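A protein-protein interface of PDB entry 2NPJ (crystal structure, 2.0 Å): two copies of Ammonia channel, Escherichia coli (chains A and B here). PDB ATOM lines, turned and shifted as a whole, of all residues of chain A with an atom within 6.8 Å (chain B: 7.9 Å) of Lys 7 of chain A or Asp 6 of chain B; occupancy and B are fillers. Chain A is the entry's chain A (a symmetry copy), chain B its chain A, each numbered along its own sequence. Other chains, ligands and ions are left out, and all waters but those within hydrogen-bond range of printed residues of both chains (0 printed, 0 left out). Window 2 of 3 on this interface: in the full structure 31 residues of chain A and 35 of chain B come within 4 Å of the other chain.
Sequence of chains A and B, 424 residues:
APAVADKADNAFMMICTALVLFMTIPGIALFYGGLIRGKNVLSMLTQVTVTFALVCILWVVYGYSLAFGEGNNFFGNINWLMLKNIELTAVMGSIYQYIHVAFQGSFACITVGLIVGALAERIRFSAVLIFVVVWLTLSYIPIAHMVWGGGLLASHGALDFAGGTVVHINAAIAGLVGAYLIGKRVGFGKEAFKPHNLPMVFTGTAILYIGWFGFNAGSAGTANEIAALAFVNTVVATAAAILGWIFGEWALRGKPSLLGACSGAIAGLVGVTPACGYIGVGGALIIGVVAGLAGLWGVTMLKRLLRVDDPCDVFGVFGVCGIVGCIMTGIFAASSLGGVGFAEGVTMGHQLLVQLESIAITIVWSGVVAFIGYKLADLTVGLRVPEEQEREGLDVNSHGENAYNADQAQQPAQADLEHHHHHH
The side-chain carboxylate of Asp 6 of chain B lies within salt-bridge range of the side-chain amino group of Lys 7 of chain A, 3.4 Å away.
The side-chain amino group of Lys 7 of chain A lies within salt-bridge range of the side-chain carboxylate of Asp 9 of chain B (2.8 Å).
The backbone carbonyl oxygen (O) of Ala 223 of chain B lies within hydrogen-bond range of the side-chain amide nitrogen (ND2) of Asn 10 of chain A, at 3.1 Å.
Of chain B, only Asp 6, Ala 8, Asp 9, Thr 222 and Ala 223 come within 4 Å of Lys 7 of chain A.
Of the printed residues of chain B, Asn 10 of chain A touches Ala 223.
Val 4 of chain B touches none of the printed residues of chain A.
Of chain A, only Lys 7 (3.4 Å) comes within 4 Å of Asp 6 of chain B.
Of the printed residues of chain A, Glu 225 of chain B touches Tyr 96.
The nearest residue of chain B that does not touch Lys 7 of chain A is Ser 94 of chain B (4.7 Å).
The nearest printed residue of chain A that does not touch Asn 224 of chain B is Asn 10 of chain A (4.4 Å).
N of Asp 9 of chain B is in hydrogen-bond range of OD1 of Asp 6 of chain B, 3.1 Å away.
The backbone carbonyl oxygen (O) of Ser 94 of chain B lies within hydrogen-bond range of the backbone NH (N) of Asp 6 of chain B, at 2.9 Å.
The side-chain carboxylate of Asp 9 of chain B sits at hydrogen-bond distance from the side-chain hydroxyl of Ser 94 of chain B (2.6 Å).
The side-chain carboxylate (OD1) of Asp 9 of chain B sits at hydrogen-bond distance from the side-chain hydroxyl (OG1) of Thr 222 of chain B (2.7 Å).
The side-chain carboxylate of Asp 9 of chain B is in hydrogen-bond range of the backbone NH of Ala 223 of chain B (2.9 Å).
The side-chain amide oxygen (OD1) of Asn 10 of chain A lies within hydrogen-bond range of the backbone NH (N) of Tyr 96 of chain A, 3.1 Å away.
C of Lys 7 of chain A touches CB of Ala 8 of chain B, at 3.6 Å.
Lys 7 of chain A touches Thr 222 of chain B (CE to OG1, 3.2 Å).
Ala 8 of chain A touches Ala 8 of chain B.
Ala 11 of chain A touches Ala 8 of chain B (CB to O, 3.9 Å).
CB of Ala 11 of chain A touches CB of Phe 12 of chain B, at 3.8 Å.
Ala 11 of chain A touches Ala 223 of chain B.
CE of Met 14 of chain A touches CE1 of Phe 12 of chain B, 3.7 Å away.
Ala 223 of chain B touches Met 14 of chain A (CB to CE, 3.9 Å).
Tyr 96 of chain A touches Asn 224 of chain B.
CE2 of Tyr 96 of chain A touches N of Glu 225 of chain B (3.3 Å).
Of the 22 printed residues of chain B, 8 touch a printed residue of chain A.
Printed residues of chain B that touch a printed residue of chain A: Asp 6, Ala 8, Asp 9, Phe 12, Thr 222, Ala 223, Asn 224 and Glu 225.
Lys 7 of chain A touches Asp 6 of chain B, but with the chains exchanged Asp 6 of chain A does not touch Lys 7 of chain B (8.8 Å).
Lys 7 of chain A touches Ala 8 of chain B, but with the chains exchanged Ala 8 of chain A does not touch Lys 7 of chain B (6.5 Å).
Ala 11 of chain A touches Ala 8 of chain B, but with the chains exchanged Ala 8 of chain A does not touch Ala 11 of chain B (6.9 Å).
Ala 11 of chain A touches Phe 12 of chain B, but with the chains exchanged Phe 12 of chain A does not touch Ala 11 of chain B (7.2 Å).
Positions printed for both chains: 5, 6, 7, 8, 9, 10, 11, 12, 94 and 96.
Of the 14 pairs that touch across the chains among the printed residues, 1 has its exchanged pair printed and touching as well.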
ATOM      1  N   ALA A   5       1.774  11.822   4.934  1.00  0.00           N
ATOM      2  CA  ALA A   5       3.194  12.037   4.704  1.00  0.00           C
ATOM      3  C   ALA A   5       3.991  10.794   5.087  1.00  0.00           C
ATOM      4  O   ALA A   5       3.677  10.121   6.074  1.00  0.00           O
ATOM      5  CB  ALA A   5       3.688  13.247   5.490  1.00  0.00           C
ATOM      6  N   ASP A   6       5.004  10.490   4.284  1.00  0.00           N
ATOM      7  CA  ASP A   6       5.869   9.356   4.538  1.00  0.00           C
ATOM      8  C   ASP A   6       7.116   9.969   5.182  1.00  0.00           C
ATOM      9  O   ASP A   6       7.772  10.822   4.583  1.00  0.00           O
ATOM     10  CB  ASP A   6       6.200   8.634   3.228  1.00  0.00           C
ATOM     11  CG  ASP A   6       7.130   7.449   3.429  1.00  0.00           C
ATOM     12  OD1 ASP A   6       8.301   7.659   3.784  1.00  0.00           O
ATOM     13  OD2 ASP A   6       6.703   6.305   3.209  1.00  0.00           O
ATOM     14  N   LYS A   7       7.419   9.568   6.414  1.00  0.00           N
ATOM     15  CA  LYS A   7       8.580  10.119   7.143  1.00  0.00           C
ATOM     16  C   LYS A   7       9.917   9.894   6.432  1.00  0.00           C
ATOM     17  O   LYS A   7      10.820  10.712   6.553  1.00  0.00           O
ATOM     18  CB  LYS A   7       8.612   9.611   8.589  1.00  0.00           C
ATOM     19  CG  LYS A   7       7.540  10.264   9.466  1.00  0.00           C
ATOM     20  CD  LYS A   7       7.187   9.394  10.657  1.00  0.00           C
ATOM     21  CE  LYS A   7       8.172   9.552  11.770  1.00  0.00           C
ATOM     22  NZ  LYS A   7       7.858   8.671  12.946  1.00  0.00           N
ATOM     23  N   ALA A   8      10.037   8.800   5.686  1.00  0.00           N
ATOM     24  CA  ALA A   8      11.278   8.525   4.942  1.00  0.00           C
ATOM     25  C   ALA A   8      11.457   9.577   3.832  1.00  0.00           C
ATOM     26  O   ALA A   8      12.571  10.060   3.574  1.00  0.00           O
ATOM     27  CB  ALA A   8      11.229   7.125   4.344  1.00  0.00           C
ATOM     28  N   ASP A   9      10.348   9.933   3.181  1.00  0.00           N
ATOM     29  CA  ASP A   9      10.377  10.932   2.112  1.00  0.00           C
ATOM     30  C   ASP A   9      10.596  12.320   2.724  1.00  0.00           C
ATOM     31  O   ASP A   9      11.318  13.139   2.155  1.00  0.00           O
ATOM     32  CB  ASP A   9       9.088  10.879   1.279  1.00  0.00           C
ATOM     33  CG  ASP A   9       8.973   9.603   0.458  1.00  0.00           C
ATOM     34  OD1 ASP A   9      10.022   8.973   0.171  1.00  0.00           O
ATOM     35  OD2 ASP A   9       7.833   9.216   0.113  1.00  0.00           O
ATOM     36  N   ASN A  10       9.997  12.571   3.890  1.00  0.00           N
ATOM     37  CA  ASN A  10      10.175  13.855   4.574  1.00  0.00           C
ATOM     38  C   ASN A  10      11.662  14.048   4.889  1.00  0.00           C
ATOM     39  O   ASN A  10      12.216  15.120   4.665  1.00  0.00           O
ATOM     40  CB  ASN A  10       9.425  13.898   5.916  1.00  0.00           C
ATOM     41  CG  ASN A  10       7.916  14.061   5.770  1.00  0.00           C
ATOM     42  OD1 ASN A  10       7.413  14.546   4.760  1.00  0.00           O
ATOM     43  ND2 ASN A  10       7.190  13.672   6.809  1.00  0.00           N
ATOM     44  N   ALA A  11      12.282  13.012   5.444  1.00  0.00           N
ATOM     45  CA  ALA A  11      13.712  13.045   5.811  1.00  0.00           C
ATOM     46  C   ALA A  11      14.581  13.289   4.586  1.00  0.00           C
ATOM     47  O   ALA A  11      15.445  14.171   4.585  1.00  0.00           O
ATOM     48  CB  ALA A  11      14.117  11.710   6.497  1.00  0.00           C
ATOM     49  N   PHE A  12      14.367  12.484   3.546  1.00  0.00           N
ATOM     50  CA  PHE A  12      15.124  12.595   2.312  1.00  0.00           C
ATOM     51  C   PHE A  12      15.041  14.004   1.707  1.00  0.00           C
ATOM     52  O   PHE A  12      16.057  14.594   1.300  1.00  0.00           O
ATOM     53  CB  PHE A  12      14.579  11.574   1.293  1.00  0.00           C
ATOM     54  CG  PHE A  12      15.344  11.527  -0.004  1.00  0.00           C
ATOM     55  CD1 PHE A  12      16.705  11.210  -0.023  1.00  0.00           C
ATOM     56  CD2 PHE A  12      14.695  11.767  -1.214  1.00  0.00           C
ATOM     57  CE1 PHE A  12      17.419  11.159  -1.238  1.00  0.00           C
ATOM     58  CE2 PHE A  12      15.389  11.711  -2.423  1.00  0.00           C
ATOM     59  CZ  PHE A  12      16.758  11.408  -2.433  1.00  0.00           C
ATOM     60  N   MET A  14      14.101  16.919   3.160  1.00  0.00           N
ATOM     61  CA  MET A  14      14.670  18.000   3.977  1.00  0.00           C
ATOM     62  C   MET A  14      16.198  17.972   3.782  1.00  0.00           C
ATOM     63  O   MET A  14      16.817  19.021   3.630  1.00  0.00           O
ATOM     64  CB  MET A  14      14.318  17.857   5.459  1.00  0.00           C
ATOM     65  CG  MET A  14      12.909  18.356   5.778  1.00  0.00           C
ATOM     66  SD  MET A  14      12.536  18.364   7.544  1.00  0.00           S
ATOM     67  CE  MET A  14      12.187  16.616   7.793  1.00  0.00           C
ATOM     68  N   SER A  94       4.096  12.980  -1.255  1.00  0.00           N
ATOM     69  CA  SER A  94       4.229  12.089  -0.095  1.00  0.00           C
ATOM     70  C   SER A  94       4.982  12.771   1.056  1.00  0.00           C
ATOM     71  O   SER A  94       5.454  12.106   1.979  1.00  0.00           O
ATOM     72  CB  SER A  94       4.911  10.763  -0.476  1.00  0.00           C
ATOM     73  OG  SER A  94       6.212  10.984  -0.987  1.00  0.00           O
ATOM     74  N   TYR A  96       5.320  16.579   3.668  1.00  0.00           N
ATOM     75  CA  TYR A  96       4.597  17.740   4.188  1.00  0.00           C
ATOM     76  C   TYR A  96       4.831  18.893   3.206  1.00  0.00           C
ATOM     77  O   TYR A  96       5.938  19.070   2.694  1.00  0.00           O
ATOM     78  CB  TYR A  96       5.065  18.101   5.614  1.00  0.00           C
ATOM     79  CG  TYR A  96       4.508  17.128   6.631  1.00  0.00           C
ATOM     80  CD1 TYR A  96       3.128  16.998   6.806  1.00  0.00           C
ATOM     81  CD2 TYR A  96       5.346  16.316   7.390  1.00  0.00           C
ATOM     82  CE1 TYR A  96       2.595  16.094   7.722  1.00  0.00           C
ATOM     83  CE2 TYR A  96       4.814  15.398   8.322  1.00  0.00           C
ATOM     84  CZ  TYR A  96       3.445  15.298   8.472  1.00  0.00           C
ATOM     85  OH  TYR A  96       2.918  14.411   9.379  1.00  0.00           O
ATOM     86  N   ALA B   3       8.062   0.867  22.859  1.00  0.00           N
ATOM     87  CA  ALA B   3       8.555   1.845  21.836  1.00  0.00           C
ATOM     88  C   ALA B   3       9.524   1.188  20.861  1.00  0.00           C
ATOM     89  O   ALA B   3      10.506   0.565  21.274  1.00  0.00           O
ATOM     90  CB  ALA B   3       9.214   3.039  22.509  1.00  0.00           C
ATOM     91  N   VAL B   4       9.227   1.321  19.569  1.00  0.00           N
ATOM     92  CA  VAL B   4      10.061   0.760  18.509  1.00  0.00           C
ATOM     93  C   VAL B   4      10.693   1.910  17.708  1.00  0.00           C
ATOM     94  O   VAL B   4      10.106   2.990  17.584  1.00  0.00           O
ATOM     95  CB  VAL B   4       9.266  -0.239  17.605  1.00  0.00           C
ATOM     96  CG1 VAL B   4       8.196   0.474  16.775  1.00  0.00           C
ATOM     97  CG2 VAL B   4      10.198  -1.026  16.704  1.00  0.00           C
ATOM     98  N   ALA B   5      11.908   1.695  17.209  1.00  0.00           N
ATOM     99  CA  ALA B   5      12.593   2.728  16.449  1.00  0.00           C
ATOM    100  C   ALA B   5      12.022   2.820  15.037  1.00  0.00           C
ATOM    101  O   ALA B   5      11.685   1.803  14.424  1.00  0.00           O
ATOM    102  CB  ALA B   5      14.092   2.453  16.398  1.00  0.00           C
ATOM    103  N   ASP B   6      11.897   4.047  14.546  1.00  0.00           N
ATOM    104  CA  ASP B   6      11.399   4.290  13.207  1.00  0.00           C
ATOM    105  C   ASP B   6      12.660   4.539  12.375  1.00  0.00           C
ATOM    106  O   ASP B   6      13.428   5.457  12.667  1.00  0.00           O
ATOM    107  CB  ASP B   6      10.460   5.500  13.199  1.00  0.00           C
ATOM    108  CG  ASP B   6       9.928   5.821  11.812  1.00  0.00           C
ATOM    109  OD1 ASP B   6      10.716   6.237  10.948  1.00  0.00           O
ATOM    110  OD2 ASP B   6       8.715   5.682  11.586  1.00  0.00           O
ATOM    111  N   LYS B   7      12.894   3.703  11.366  1.00  0.00           N
ATOM    112  CA  LYS B   7      14.098   3.831  10.521  1.00  0.00           C
ATOM    113  C   LYS B   7      14.208   5.179   9.803  1.00  0.00           C
ATOM    114  O   LYS B   7      15.309   5.659   9.568  1.00  0.00           O
ATOM    115  CB  LYS B   7      14.208   2.656   9.542  1.00  0.00           C
ATOM    116  CG  LYS B   7      14.627   1.353  10.230  1.00  0.00           C
ATOM    117  CD  LYS B   7      14.182   0.137   9.440  1.00  0.00           C
ATOM    118  CE  LYS B   7      15.123  -0.170   8.319  1.00  0.00           C
ATOM    119  NZ  LYS B   7      14.680  -1.353   7.505  1.00  0.00           N
ATOM    120  N   ALA B   8      13.074   5.790   9.474  1.00  0.00           N
ATOM    121  CA  ALA B   8      13.090   7.106   8.812  1.00  0.00           C
ATOM    122  C   ALA B   8      13.643   8.164   9.783  1.00  0.00           C
ATOM    123  O   ALA B   8      14.416   9.056   9.395  1.00  0.00           O
ATOM    124  CB  ALA B   8      11.683   7.482   8.361  1.00  0.00           C
ATOM    125  N   ASP B   9      13.247   8.056  11.052  1.00  0.00           N
ATOM    126  CA  ASP B   9      13.709   8.990  12.080  1.00  0.00           C
ATOM    127  C   ASP B   9      15.180   8.703  12.399  1.00  0.00           C
ATOM    128  O   ASP B   9      15.958   9.632  12.612  1.00  0.00           O
ATOM    129  CB  ASP B   9      12.831   8.898  13.336  1.00  0.00           C
ATOM    130  CG  ASP B   9      11.420   9.421  13.105  1.00  0.00           C
ATOM    131  OD1 ASP B   9      11.224  10.236  12.168  1.00  0.00           O
ATOM    132  OD2 ASP B   9      10.500   9.007  13.846  1.00  0.00           O
ATOM    133  N   ASN B  10      15.562   7.423  12.404  1.00  0.00           N
ATOM    134  CA  ASN B  10      16.956   7.048  12.660  1.00  0.00           C
ATOM    135  C   ASN B  10      17.846   7.682  11.587  1.00  0.00           C
ATOM    136  O   ASN B  10      18.891   8.249  11.892  1.00  0.00           O
ATOM    137  CB  ASN B  10      17.164   5.528  12.574  1.00  0.00           C
ATOM    138  CG  ASN B  10      16.623   4.765  13.779  1.00  0.00           C
ATOM    139  OD1 ASN B  10      16.456   5.309  14.867  1.00  0.00           O
ATOM    140  ND2 ASN B  10      16.372   3.478  13.581  1.00  0.00           N
ATOM    141  N   ALA B  11      17.437   7.542  10.330  1.00  0.00           N
ATOM    142  CA  ALA B  11      18.189   8.091   9.184  1.00  0.00           C
ATOM    143  C   ALA B  11      18.312   9.604   9.289  1.00  0.00           C
ATOM    144  O   ALA B  11      19.406  10.163   9.172  1.00  0.00           O
ATOM    145  CB  ALA B  11      17.488   7.702   7.851  1.00  0.00           C
ATOM    146  N   PHE B  12      17.175  10.271   9.486  1.00  0.00           N
ATOM    147  CA  PHE B  12      17.137  11.718   9.601  1.00  0.00           C
ATOM    148  C   PHE B  12      18.061  12.235  10.712  1.00  0.00           C
ATOM    149  O   PHE B  12      18.829  13.195  10.521  1.00  0.00           O
ATOM    150  CB  PHE B  12      15.690  12.162   9.900  1.00  0.00           C
ATOM    151  CG  PHE B  12      15.500  13.655   9.953  1.00  0.00           C
ATOM    152  CD1 PHE B  12      15.792  14.455   8.845  1.00  0.00           C
ATOM    153  CD2 PHE B  12      14.996  14.261  11.102  1.00  0.00           C
ATOM    154  CE1 PHE B  12      15.607  15.852   8.892  1.00  0.00           C
ATOM    155  CE2 PHE B  12      14.801  15.642  11.158  1.00  0.00           C
ATOM    156  CZ  PHE B  12      15.110  16.440  10.047  1.00  0.00           C
ATOM    157  N   MET B  13      17.969  11.598  11.874  1.00  0.00           N
ATOM    158  CA  MET B  13      18.736  11.999  13.058  1.00  0.00           C
ATOM    159  C   MET B  13      20.234  11.736  12.971  1.00  0.00           C
ATOM    160  O   MET B  13      21.027  12.508  13.511  1.00  0.00           O
ATOM    161  CB  MET B  13      18.079  11.427  14.330  1.00  0.00           C
ATOM    162  CG  MET B  13      16.676  12.028  14.590  1.00  0.00           C
ATOM    163  SD  MET B  13      16.714  13.846  14.794  1.00  0.00           S
ATOM    164  CE  MET B  13      17.754  14.004  16.249  1.00  0.00           C
ATOM    165  N   VAL B  91      15.449   2.314  22.702  1.00  0.00           N
ATOM    166  CA  VAL B  91      14.830   3.429  21.975  1.00  0.00           C
ATOM    167  C   VAL B  91      14.571   4.644  22.870  1.00  0.00           C
ATOM    168  O   VAL B  91      14.108   4.504  24.009  1.00  0.00           O
ATOM    169  CB  VAL B  91      13.475   2.965  21.344  1.00  0.00           C
ATOM    170  CG1 VAL B  91      12.758   4.099  20.597  1.00  0.00           C
ATOM    171  CG2 VAL B  91      13.691   1.765  20.430  1.00  0.00           C
ATOM    172  N   GLY B  93      12.486   8.097  22.392  1.00  0.00           N
ATOM    173  CA  GLY B  93      11.576   8.804  21.476  1.00  0.00           C
ATOM    174  C   GLY B  93      11.209   7.824  20.381  1.00  0.00           C
ATOM    175  O   GLY B  93      10.605   6.797  20.667  1.00  0.00           O
ATOM    176  N   SER B  94      11.606   8.115  19.137  1.00  0.00           N
ATOM    177  CA  SER B  94      11.335   7.209  18.013  1.00  0.00           C
ATOM    178  C   SER B  94      12.631   6.764  17.323  1.00  0.00           C
ATOM    179  O   SER B  94      12.603   6.261  16.199  1.00  0.00           O
ATOM    180  CB  SER B  94      10.371   7.844  16.994  1.00  0.00           C
ATOM    181  OG  SER B  94      10.910   9.036  16.452  1.00  0.00           O
ATOM    182  N   ILE B  95      13.764   6.966  17.993  1.00  0.00           N
ATOM    183  CA  ILE B  95      15.067   6.590  17.436  1.00  0.00           C
ATOM    184  C   ILE B  95      15.872   5.766  18.431  1.00  0.00           C
ATOM    185  O   ILE B  95      15.576   5.768  19.634  1.00  0.00           O
ATOM    186  CB  ILE B  95      15.915   7.850  17.022  1.00  0.00           C
ATOM    187  CG1 ILE B  95      16.273   8.711  18.250  1.00  0.00           C
ATOM    188  CG2 ILE B  95      15.191   8.668  15.956  1.00  0.00           C
ATOM    189  CD1 ILE B  95      17.283   9.859  17.971  1.00  0.00           C
ATOM    190  N   TYR B  96      16.895   5.069  17.941  1.00  0.00           N
ATOM    191  CA  TYR B  96      17.754   4.289  18.832  1.00  0.00           C
ATOM    192  C   TYR B  96      18.461   5.281  19.761  1.00  0.00           C
ATOM    193  O   TYR B  96      18.883   6.356  19.330  1.00  0.00           O
ATOM    194  CB  TYR B  96      18.763   3.435  18.036  1.00  0.00           C
ATOM    195  CG  TYR B  96      18.087   2.233  17.413  1.00  0.00           C
ATOM    196  CD1 TYR B  96      17.470   1.272  18.217  1.00  0.00           C
ATOM    197  CD2 TYR B  96      18.029   2.070  16.031  1.00  0.00           C
ATOM    198  CE1 TYR B  96      16.824   0.168  17.662  1.00  0.00           C
ATOM    199  CE2 TYR B  96      17.376   0.954  15.462  1.00  0.00           C
ATOM    200  CZ  TYR B  96      16.780   0.020  16.286  1.00  0.00           C
ATOM    201  OH  TYR B  96      16.147  -1.070  15.741  1.00  0.00           O
ATOM    202  N   ILE B  99      21.710   6.989  18.861  1.00  0.00           N
ATOM    203  CA  ILE B  99      21.634   8.155  17.964  1.00  0.00           C
ATOM    204  C   ILE B  99      21.385   9.422  18.806  1.00  0.00           C
ATOM    205  O   ILE B  99      21.970  10.476  18.543  1.00  0.00           O
ATOM    206  CB  ILE B  99      20.557   7.984  16.867  1.00  0.00           C
ATOM    207  CG1 ILE B  99      20.868   6.743  16.019  1.00  0.00           C
ATOM    208  CG2 ILE B  99      20.505   9.235  15.978  1.00  0.00           C
ATOM    209  CD1 ILE B  99      19.779   6.369  14.994  1.00  0.00           C
ATOM    210  N   GLY B 221      13.517  15.630  16.634  1.00  0.00           N
ATOM    211  CA  GLY B 221      13.767  14.215  16.953  1.00  0.00           C
ATOM    212  C   GLY B 221      13.090  13.225  16.016  1.00  0.00           C
ATOM    213  O   GLY B 221      13.118  12.014  16.251  1.00  0.00           O
ATOM    214  N   THR B 222      12.497  13.740  14.942  1.00  0.00           N
ATOM    215  CA  THR B 222      11.765  12.931  13.968  1.00  0.00           C
ATOM    216  C   THR B 222      11.549  13.755  12.708  1.00  0.00           C
ATOM    217  O   THR B 222      11.498  14.983  12.780  1.00  0.00           O
ATOM    218  CB  THR B 222      10.365  12.502  14.542  1.00  0.00           C
ATOM    219  OG1 THR B 222       9.547  11.916  13.511  1.00  0.00           O
ATOM    220  CG2 THR B 222       9.620  13.691  15.177  1.00  0.00           C
ATOM    221  N   ALA B 223      11.407  13.083  11.564  1.00  0.00           N
ATOM    222  CA  ALA B 223      11.178  13.786  10.303  1.00  0.00           C
ATOM    223  C   ALA B 223       9.674  13.997  10.121  1.00  0.00           C
ATOM    224  O   ALA B 223       9.043  13.393   9.246  1.00  0.00           O
ATOM    225  CB  ALA B 223      11.794  13.003   9.131  1.00  0.00           C
ATOM    226  N   ASN B 224       9.099  14.835  10.988  1.00  0.00           N
ATOM    227  CA  ASN B 224       7.673  15.131  10.967  1.00  0.00           C
ATOM    228  C   ASN B 224       7.377  16.580  10.544  1.00  0.00           C
ATOM    229  O   ASN B 224       8.239  17.259   9.983  1.00  0.00           O
ATOM    230  CB  ASN B 224       7.033  14.809  12.337  1.00  0.00           C
ATOM    231  CG  ASN B 224       7.467  15.779  13.440  1.00  0.00           C
ATOM    232  OD1 ASN B 224       8.429  16.532  13.280  1.00  0.00           O
ATOM    233  ND2 ASN B 224       6.753  15.753  14.571  1.00  0.00           N
ATOM    234  N   GLU B 225       6.160  17.039  10.819  1.00  0.00           N
ATOM    235  CA  GLU B 225       5.749  18.399  10.454  1.00  0.00           C
ATOM    236  C   GLU B 225       6.444  19.487  11.286  1.00  0.00           C
ATOM    237  O   GLU B 225       6.550  20.625  10.837  1.00  0.00           O
ATOM    238  CB  GLU B 225       4.220  18.543  10.499  1.00  0.00           C
ATOM    239  CG  GLU B 225       3.604  18.674  11.894  1.00  0.00           C
ATOM    240  CD  GLU B 225       3.455  17.348  12.624  1.00  0.00           C
ATOM    241  OE1 GLU B 225       3.955  16.299  12.143  1.00  0.00           O
ATOM    242  OE2 GLU B 225       2.823  17.360  13.691  1.00  0.00           O
